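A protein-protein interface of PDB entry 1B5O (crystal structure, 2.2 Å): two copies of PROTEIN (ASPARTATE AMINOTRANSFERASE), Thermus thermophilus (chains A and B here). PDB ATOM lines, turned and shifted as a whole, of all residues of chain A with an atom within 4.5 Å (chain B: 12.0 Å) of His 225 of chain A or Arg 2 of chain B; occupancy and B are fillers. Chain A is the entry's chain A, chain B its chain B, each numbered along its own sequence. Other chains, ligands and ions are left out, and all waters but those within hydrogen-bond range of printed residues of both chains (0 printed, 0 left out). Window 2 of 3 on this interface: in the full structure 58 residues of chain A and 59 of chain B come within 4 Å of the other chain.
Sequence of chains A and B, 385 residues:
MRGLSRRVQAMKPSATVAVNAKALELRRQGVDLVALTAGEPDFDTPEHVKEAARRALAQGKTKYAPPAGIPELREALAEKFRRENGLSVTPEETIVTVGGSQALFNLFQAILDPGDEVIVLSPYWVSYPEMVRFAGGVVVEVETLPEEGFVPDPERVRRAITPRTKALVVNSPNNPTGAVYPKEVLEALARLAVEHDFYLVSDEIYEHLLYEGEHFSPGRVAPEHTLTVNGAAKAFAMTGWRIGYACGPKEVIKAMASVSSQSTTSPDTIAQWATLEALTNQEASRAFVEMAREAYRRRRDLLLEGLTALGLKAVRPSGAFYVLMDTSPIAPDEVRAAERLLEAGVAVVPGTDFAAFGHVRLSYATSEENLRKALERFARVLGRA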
ATOM      1  N   LYS A 166       6.232  16.729  -0.364  1.00  0.00           N
ATOM      2  CA  LYS A 166       6.922  16.080   0.748  1.00  0.00           C
ATOM      3  C   LYS A 166       6.929  16.945   2.010  1.00  0.00           C
ATOM      4  O   LYS A 166       6.930  16.419   3.129  1.00  0.00           O
ATOM      5  CB  LYS A 166       8.362  15.757   0.346  1.00  0.00           C
ATOM      6  CG  LYS A 166       8.672  14.280   0.285  1.00  0.00           C
ATOM      7  CD  LYS A 166       8.739  13.678   1.677  1.00  0.00           C
ATOM      8  CE  LYS A 166       8.909  12.159   1.642  1.00  0.00           C
ATOM      9  NZ  LYS A 166      10.197  11.711   1.032  1.00  0.00           N
ATOM     10  N   ALA A 193      -1.299  19.144   6.597  1.00  0.00           N
ATOM     11  CA  ALA A 193      -0.160  18.226   6.619  1.00  0.00           C
ATOM     12  C   ALA A 193      -0.636  16.824   6.975  1.00  0.00           C
ATOM     13  O   ALA A 193      -0.255  15.854   6.327  1.00  0.00           O
ATOM     14  CB  ALA A 193       0.891  18.698   7.632  1.00  0.00           C
ATOM     15  N   VAL A 194      -1.485  16.739   8.000  1.00  0.00           N
ATOM     16  CA  VAL A 194      -2.040  15.470   8.466  1.00  0.00           C
ATOM     17  C   VAL A 194      -3.048  14.892   7.469  1.00  0.00           C
ATOM     18  O   VAL A 194      -3.060  13.692   7.209  1.00  0.00           O
ATOM     19  CB  VAL A 194      -2.733  15.636   9.839  1.00  0.00           C
ATOM     20  CG1 VAL A 194      -3.333  14.310  10.289  1.00  0.00           C
ATOM     21  CG2 VAL A 194      -1.741  16.132  10.871  1.00  0.00           C
ATOM     22  N   ASP A 197      -0.954  13.979   4.356  1.00  0.00           N
ATOM     23  CA  ASP A 197       0.230  13.188   4.697  1.00  0.00           C
ATOM     24  C   ASP A 197       1.580  13.728   4.202  1.00  0.00           C
ATOM     25  O   ASP A 197       2.107  13.277   3.185  1.00  0.00           O
ATOM     26  CB  ASP A 197       0.021  11.735   4.228  1.00  0.00           C
ATOM     27  CG  ASP A 197       1.075  10.781   4.758  1.00  0.00           C
ATOM     28  OD1 ASP A 197       1.318  10.761   5.983  1.00  0.00           O
ATOM     29  OD2 ASP A 197       1.644  10.029   3.944  1.00  0.00           O
ATOM     30  N   PHE A 198       2.115  14.720   4.902  1.00  0.00           N
ATOM     31  CA  PHE A 198       3.415  15.275   4.559  1.00  0.00           C
ATOM     32  C   PHE A 198       4.015  16.005   5.745  1.00  0.00           C
ATOM     33  O   PHE A 198       3.354  16.168   6.777  1.00  0.00           O
ATOM     34  CB  PHE A 198       3.388  16.133   3.271  1.00  0.00           C
ATOM     35  CG  PHE A 198       2.590  17.414   3.366  1.00  0.00           C
ATOM     36  CD1 PHE A 198       2.967  18.438   4.234  1.00  0.00           C
ATOM     37  CD2 PHE A 198       1.487  17.615   2.544  1.00  0.00           C
ATOM     38  CE1 PHE A 198       2.263  19.637   4.283  1.00  0.00           C
ATOM     39  CE2 PHE A 198       0.777  18.816   2.586  1.00  0.00           C
ATOM     40  CZ  PHE A 198       1.169  19.828   3.461  1.00  0.00           C
ATOM     41  N   TYR A 199       5.282  16.389   5.622  1.00  0.00           N
ATOM     42  CA  TYR A 199       5.979  17.082   6.704  1.00  0.00           C
ATOM     43  C   TYR A 199       5.767  18.589   6.760  1.00  0.00           C
ATOM     44  O   TYR A 199       5.769  19.273   5.739  1.00  0.00           O
ATOM     45  CB  TYR A 199       7.488  16.820   6.641  1.00  0.00           C
ATOM     46  CG  TYR A 199       7.892  15.386   6.854  1.00  0.00           C
ATOM     47  CD1 TYR A 199       7.734  14.771   8.097  1.00  0.00           C
ATOM     48  CD2 TYR A 199       8.470  14.654   5.820  1.00  0.00           C
ATOM     49  CE1 TYR A 199       8.150  13.454   8.304  1.00  0.00           C
ATOM     50  CE2 TYR A 199       8.889  13.340   6.014  1.00  0.00           C
ATOM     51  CZ  TYR A 199       8.727  12.744   7.255  1.00  0.00           C
ATOM     52  OH  TYR A 199       9.143  11.440   7.435  1.00  0.00           O
ATOM     53  N   LEU A 200       5.623  19.088   7.980  1.00  0.00           N
ATOM     54  CA  LEU A 200       5.461  20.505   8.235  1.00  0.00           C
ATOM     55  C   LEU A 200       6.747  20.908   8.959  1.00  0.00           C
ATOM     56  O   LEU A 200       7.077  20.363  10.015  1.00  0.00           O
ATOM     57  CB  LEU A 200       4.241  20.746   9.128  1.00  0.00           C
ATOM     58  CG  LEU A 200       3.490  22.087   9.108  1.00  0.00           C
ATOM     59  CD1 LEU A 200       3.407  22.649  10.511  1.00  0.00           C
ATOM     60  CD2 LEU A 200       4.141  23.082   8.175  1.00  0.00           C
ATOM     61  N   ALA A 222       0.146  18.531  15.478  1.00  0.00           N
ATOM     62  CA  ALA A 222       0.573  17.484  14.538  1.00  0.00           C
ATOM     63  C   ALA A 222       1.994  17.006  14.825  1.00  0.00           C
ATOM     64  O   ALA A 222       2.881  17.144  13.985  1.00  0.00           O
ATOM     65  CB  ALA A 222       0.472  17.991  13.099  1.00  0.00           C
ATOM     66  N   PRO A 223       2.211  16.383  15.995  1.00  0.00           N
ATOM     67  CA  PRO A 223       3.520  15.873  16.420  1.00  0.00           C
ATOM     68  C   PRO A 223       4.252  14.907  15.482  1.00  0.00           C
ATOM     69  O   PRO A 223       5.465  15.020  15.307  1.00  0.00           O
ATOM     70  CB  PRO A 223       3.218  15.244  17.787  1.00  0.00           C
ATOM     71  CG  PRO A 223       1.764  14.876  17.695  1.00  0.00           C
ATOM     72  CD  PRO A 223       1.181  16.076  17.006  1.00  0.00           C
ATOM     73  N   GLU A 224       3.525  13.976  14.872  1.00  0.00           N
ATOM     74  CA  GLU A 224       4.134  13.001  13.964  1.00  0.00           C
ATOM     75  C   GLU A 224       4.475  13.575  12.597  1.00  0.00           C
ATOM     76  O   GLU A 224       5.189  12.944  11.817  1.00  0.00           O
ATOM     77  CB  GLU A 224       3.222  11.782  13.783  1.00  0.00           C
ATOM     78  CG  GLU A 224       3.500  10.613  14.724  1.00  0.00           C
ATOM     79  CD  GLU A 224       3.194  10.930  16.177  1.00  0.00           C
ATOM     80  OE1 GLU A 224       1.995  10.966  16.542  1.00  0.00           O
ATOM     81  OE2 GLU A 224       4.156  11.133  16.955  1.00  0.00           O
ATOM     82  N   HIS A 225       3.952  14.762  12.303  1.00  0.00           N
ATOM     83  CA  HIS A 225       4.200  15.406  11.017  1.00  0.00           C
ATOM     84  C   HIS A 225       5.049  16.675  11.127  1.00  0.00           C
ATOM     85  O   HIS A 225       5.397  17.263  10.108  1.00  0.00           O
ATOM     86  CB  HIS A 225       2.873  15.803  10.358  1.00  0.00           C
ATOM     87  CG  HIS A 225       1.967  14.650  10.045  1.00  0.00           C
ATOM     88  ND1 HIS A 225       1.318  13.922  11.020  1.00  0.00           N
ATOM     89  CD2 HIS A 225       1.571  14.130   8.860  1.00  0.00           C
ATOM     90  CE1 HIS A 225       0.560  13.003  10.449  1.00  0.00           C
ATOM     91  NE2 HIS A 225       0.695  13.108   9.140  1.00  0.00           N
ATOM     92  N   THR A 226       5.413  17.081  12.341  1.00  0.00           N
ATOM     93  CA  THR A 226       6.150  18.333  12.501  1.00  0.00           C
ATOM     94  C   THR A 226       7.600  18.299  12.976  1.00  0.00           C
ATOM     95  O   THR A 226       7.934  17.692  13.981  1.00  0.00           O
ATOM     96  CB  THR A 226       5.359  19.309  13.416  1.00  0.00           C
ATOM     97  OG1 THR A 226       3.992  19.361  12.985  1.00  0.00           O
ATOM     98  CG2 THR A 226       5.954  20.722  13.356  1.00  0.00           C
ATOM     99  N   LEU A 227       8.446  19.008  12.243  1.00  0.00           N
ATOM    100  CA  LEU A 227       9.858  19.134  12.576  1.00  0.00           C
ATOM    101  C   LEU A 227      10.032  20.585  13.014  1.00  0.00           C
ATOM    102  O   LEU A 227       9.846  21.511  12.218  1.00  0.00           O
ATOM    103  CB  LEU A 227      10.714  18.841  11.343  1.00  0.00           C
ATOM    104  CG  LEU A 227      10.527  17.416  10.824  1.00  0.00           C
ATOM    105  CD1 LEU A 227      10.938  17.298   9.363  1.00  0.00           C
ATOM    106  CD2 LEU A 227      11.310  16.471  11.715  1.00  0.00           C
ATOM    107  N   MET B   1       3.453  13.178   0.903  1.00  0.00           N
ATOM    108  CA  MET B   1       3.895  11.869   1.464  1.00  0.00           C
ATOM    109  C   MET B   1       5.071  12.018   2.426  1.00  0.00           C
ATOM    110  O   MET B   1       5.871  12.940   2.302  1.00  0.00           O
ATOM    111  CB  MET B   1       4.263  10.904   0.339  1.00  0.00           C
ATOM    112  CG  MET B   1       4.722   9.546   0.835  1.00  0.00           C
ATOM    113  SD  MET B   1       3.680   8.970   2.193  1.00  0.00           S
ATOM    114  CE  MET B   1       2.405   8.075   1.283  1.00  0.00           C
ATOM    115  N   ARG B   2       5.149  11.123   3.405  1.00  0.00           N
ATOM    116  CA  ARG B   2       6.234  11.135   4.373  1.00  0.00           C
ATOM    117  C   ARG B   2       7.195   9.978   4.095  1.00  0.00           C
ATOM    118  O   ARG B   2       6.909   9.111   3.268  1.00  0.00           O
ATOM    119  CB  ARG B   2       5.682  11.043   5.791  1.00  0.00           C
ATOM    120  CG  ARG B   2       5.055  12.336   6.281  1.00  0.00           C
ATOM    121  CD  ARG B   2       4.560  12.210   7.710  1.00  0.00           C
ATOM    122  NE  ARG B   2       3.494  11.216   7.823  1.00  0.00           N
ATOM    123  CZ  ARG B   2       3.120  10.644   8.963  1.00  0.00           C
ATOM    124  NH1 ARG B   2       3.723  10.960  10.101  1.00  0.00           N
ATOM    125  NH2 ARG B   2       2.138   9.756   8.964  1.00  0.00           N
ATOM    126  N   GLY B   3       8.340   9.981   4.770  1.00  0.00           N
ATOM    127  CA  GLY B   3       9.320   8.927   4.576  1.00  0.00           C
ATOM    128  C   GLY B   3      10.706   9.469   4.289  1.00  0.00           C
ATOM    129  O   GLY B   3      10.850  10.508   3.642  1.00  0.00           O
ATOM    130  N   LEU B   4      11.727   8.750   4.746  1.00  0.00           N
ATOM    131  CA  LEU B   4      13.117   9.156   4.553  1.00  0.00           C
ATOM    132  C   LEU B   4      13.583   9.043   3.109  1.00  0.00           C
ATOM    133  O   LEU B   4      12.978   8.342   2.300  1.00  0.00           O
ATOM    134  CB  LEU B   4      14.043   8.325   5.448  1.00  0.00           C
ATOM    135  CG  LEU B   4      13.790   8.380   6.958  1.00  0.00           C
ATOM    136  CD1 LEU B   4      14.708   7.390   7.656  1.00  0.00           C
ATOM    137  CD2 LEU B   4      13.989   9.796   7.502  1.00  0.00           C
ATOM    138  N   SER B   5      14.662   9.749   2.794  1.00  0.00           N
ATOM    139  CA  SER B   5      15.249   9.729   1.460  1.00  0.00           C
ATOM    140  C   SER B   5      16.069   8.450   1.281  1.00  0.00           C
ATOM    141  O   SER B   5      16.491   7.837   2.263  1.00  0.00           O
ATOM    142  CB  SER B   5      16.163  10.935   1.289  1.00  0.00           C
ATOM    143  OG  SER B   5      17.198  10.889   2.249  1.00  0.00           O
ATOM    144  N   ARG B   6      16.314   8.071   0.030  1.00  0.00           N
ATOM    145  CA  ARG B   6      17.098   6.870  -0.278  1.00  0.00           C
ATOM    146  C   ARG B   6      18.564   6.969   0.178  1.00  0.00           C
ATOM    147  O   ARG B   6      19.128   5.989   0.656  1.00  0.00           O
ATOM    148  CB  ARG B   6      17.052   6.565  -1.777  1.00  0.00           C
ATOM    149  CG  ARG B   6      15.677   6.715  -2.392  1.00  0.00           C
ATOM    150  CD  ARG B   6      15.469   5.783  -3.571  1.00  0.00           C
ATOM    151  NE  ARG B   6      14.607   4.657  -3.210  1.00  0.00           N
ATOM    152  CZ  ARG B   6      13.278   4.709  -3.187  1.00  0.00           C
ATOM    153  NH1 ARG B   6      12.644   5.830  -3.511  1.00  0.00           N
ATOM    154  NH2 ARG B   6      12.578   3.642  -2.821  1.00  0.00           N
ATOM    155  N   VAL B   8      19.878   8.447   2.792  1.00  0.00           N
ATOM    156  CA  VAL B   8      20.064   8.256   4.226  1.00  0.00           C
ATOM    157  C   VAL B   8      19.706   6.837   4.695  1.00  0.00           C
ATOM    158  O   VAL B   8      20.219   6.363   5.707  1.00  0.00           O
ATOM    159  CB  VAL B   8      19.313   9.340   5.049  1.00  0.00           C
ATOM    160  CG1 VAL B   8      17.819   9.169   4.929  1.00  0.00           C
ATOM    161  CG2 VAL B   8      19.744   9.301   6.503  1.00  0.00           C
ATOM    162  N   GLN B   9      18.848   6.149   3.949  1.00  0.00           N
ATOM    163  CA  GLN B   9      18.470   4.783   4.306  1.00  0.00           C
ATOM    164  C   GLN B   9      19.559   3.791   3.895  1.00  0.00           C
ATOM    165  O   GLN B   9      19.683   2.722   4.489  1.00  0.00           O
ATOM    166  CB  GLN B   9      17.147   4.392   3.643  1.00  0.00           C
ATOM    167  CG  GLN B   9      15.934   5.098   4.218  1.00  0.00           C
ATOM    168  CD  GLN B   9      14.635   4.670   3.558  1.00  0.00           C
ATOM    169  OE1 GLN B   9      14.398   4.947   2.378  1.00  0.00           O
ATOM    170  NE2 GLN B   9      13.776   4.005   4.324  1.00  0.00           N
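NZ of Lys 166 of chain A lies within hydrogen-bond range of O of Gly 3 of chain B, 2.9 Å away.
O of Asp 197 of chain A is in hydrogen-bond range of N of Met 1 of chain B, at 2.7 Å.
OD1 of Asp 197 of chain A lies within salt-bridge range of NE of Arg 2 of chain B.
N of Gly 3 of chain B is in hydrogen-bond range of OH of Tyr 199 of chain A, at 3.1 Å.
The guanidinium group (NH1) of Arg 2 of chain B lies within hydrogen-bond range of the backbone carbonyl oxygen (O) of Glu 224 of chain A (3.0 Å).
The backbone NH of Tyr 199 of chain A is in hydrogen-bond range of the backbone carbonyl oxygen of Lys 166 of chain A, 3.0 Å away.
N of Phe 198 of chain A lies within hydrogen-bond range of O of Ala 193 of chain A, at 3.0 Å.
The backbone NH (N) of Leu 200 of chain A sits at hydrogen-bond distance from the backbone carbonyl oxygen (O) of His 225 of chain A.
Met 1 of chain B touches Lys 166 of chain A (O to CD, 3.0 Å).
CE of Lys 166 of chain A touches C of Arg 2 of chain B, 3.7 Å away.
CB of Phe 198 of chain A touches N of Met 1 of chain B, at 3.8 Å.
Phe 198 of chain A touches Arg 2 of chain B (CA to CG, 3.8 Å).
Tyr 199 of chain A touches Arg 2 of chain B.
CZ of Arg 2 of chain B touches NE2 of His 225 of chain A (3.5 Å).
Printed residues of chain A within 4 Å of Arg 2 of chain B: Lys 166, Asp 197, Phe 198, Tyr 199, Glu 224 and His 225.
No residue of chain B comes within 4 Å of Val 194 of chain A.
Asp 197 of chain A touches just these residues of chain B: Met 1 and Arg 2.
Phe 198 of chain A touches just these residues of chain B: Met 1 (3.8 Å) and Arg 2 (3.8 Å).
Tyr 199 of chain A touches two residues of chain B.
No residue of chain B comes within 4 Å of Leu 200 of chain A.
No residue of chain B comes within 4 Å of Ala 222 of chain A.
No residue of chain B comes within 4 Å of Pro 223 of chain A.
Glu 224 of chain A touches just one residue of chain B: Arg 2.
No residue of chain B comes within 4 Å of Thr 226 of chain A.
Of the printed residues of chain A, Gly 3 of chain B touches Lys 166 (2.9 Å) and Tyr 199 (3.1 Å).
Printed residues of chain A within 4 Å of Met 1 of chain B: Lys 166, Asp 197 and Phe 198.
Gln 9 of chain B touches none of the printed residues of chain A.
Ser 5 of chain B touches none of the printed residues of chain A.
The nearest residue of chain B that does not touch His 225 of chain A is Met 1 of chain B (7.6 Å).
Hydrophobic or aromatic side chains of chain B that line the printed part of chain A: Met 1.
Of the 13 printed residues of chain A, 6 touch a printed residue of chain B.
Hydrophobic or aromatic side chains of chain A that line the printed part of chain B: Phe 198, Tyr 199 and His 225.
Among the printed residues, Asp or Glu carboxylates within 4 Å of a Lys or Arg side-chain nitrogen of the other chain: Asp 197 of chain A with Arg 2 of chain B.
No position is printed for both chains.
Of the 11 pairs that touch across the chains among the printed residues, none has its exchanged pair printed and touching as well.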
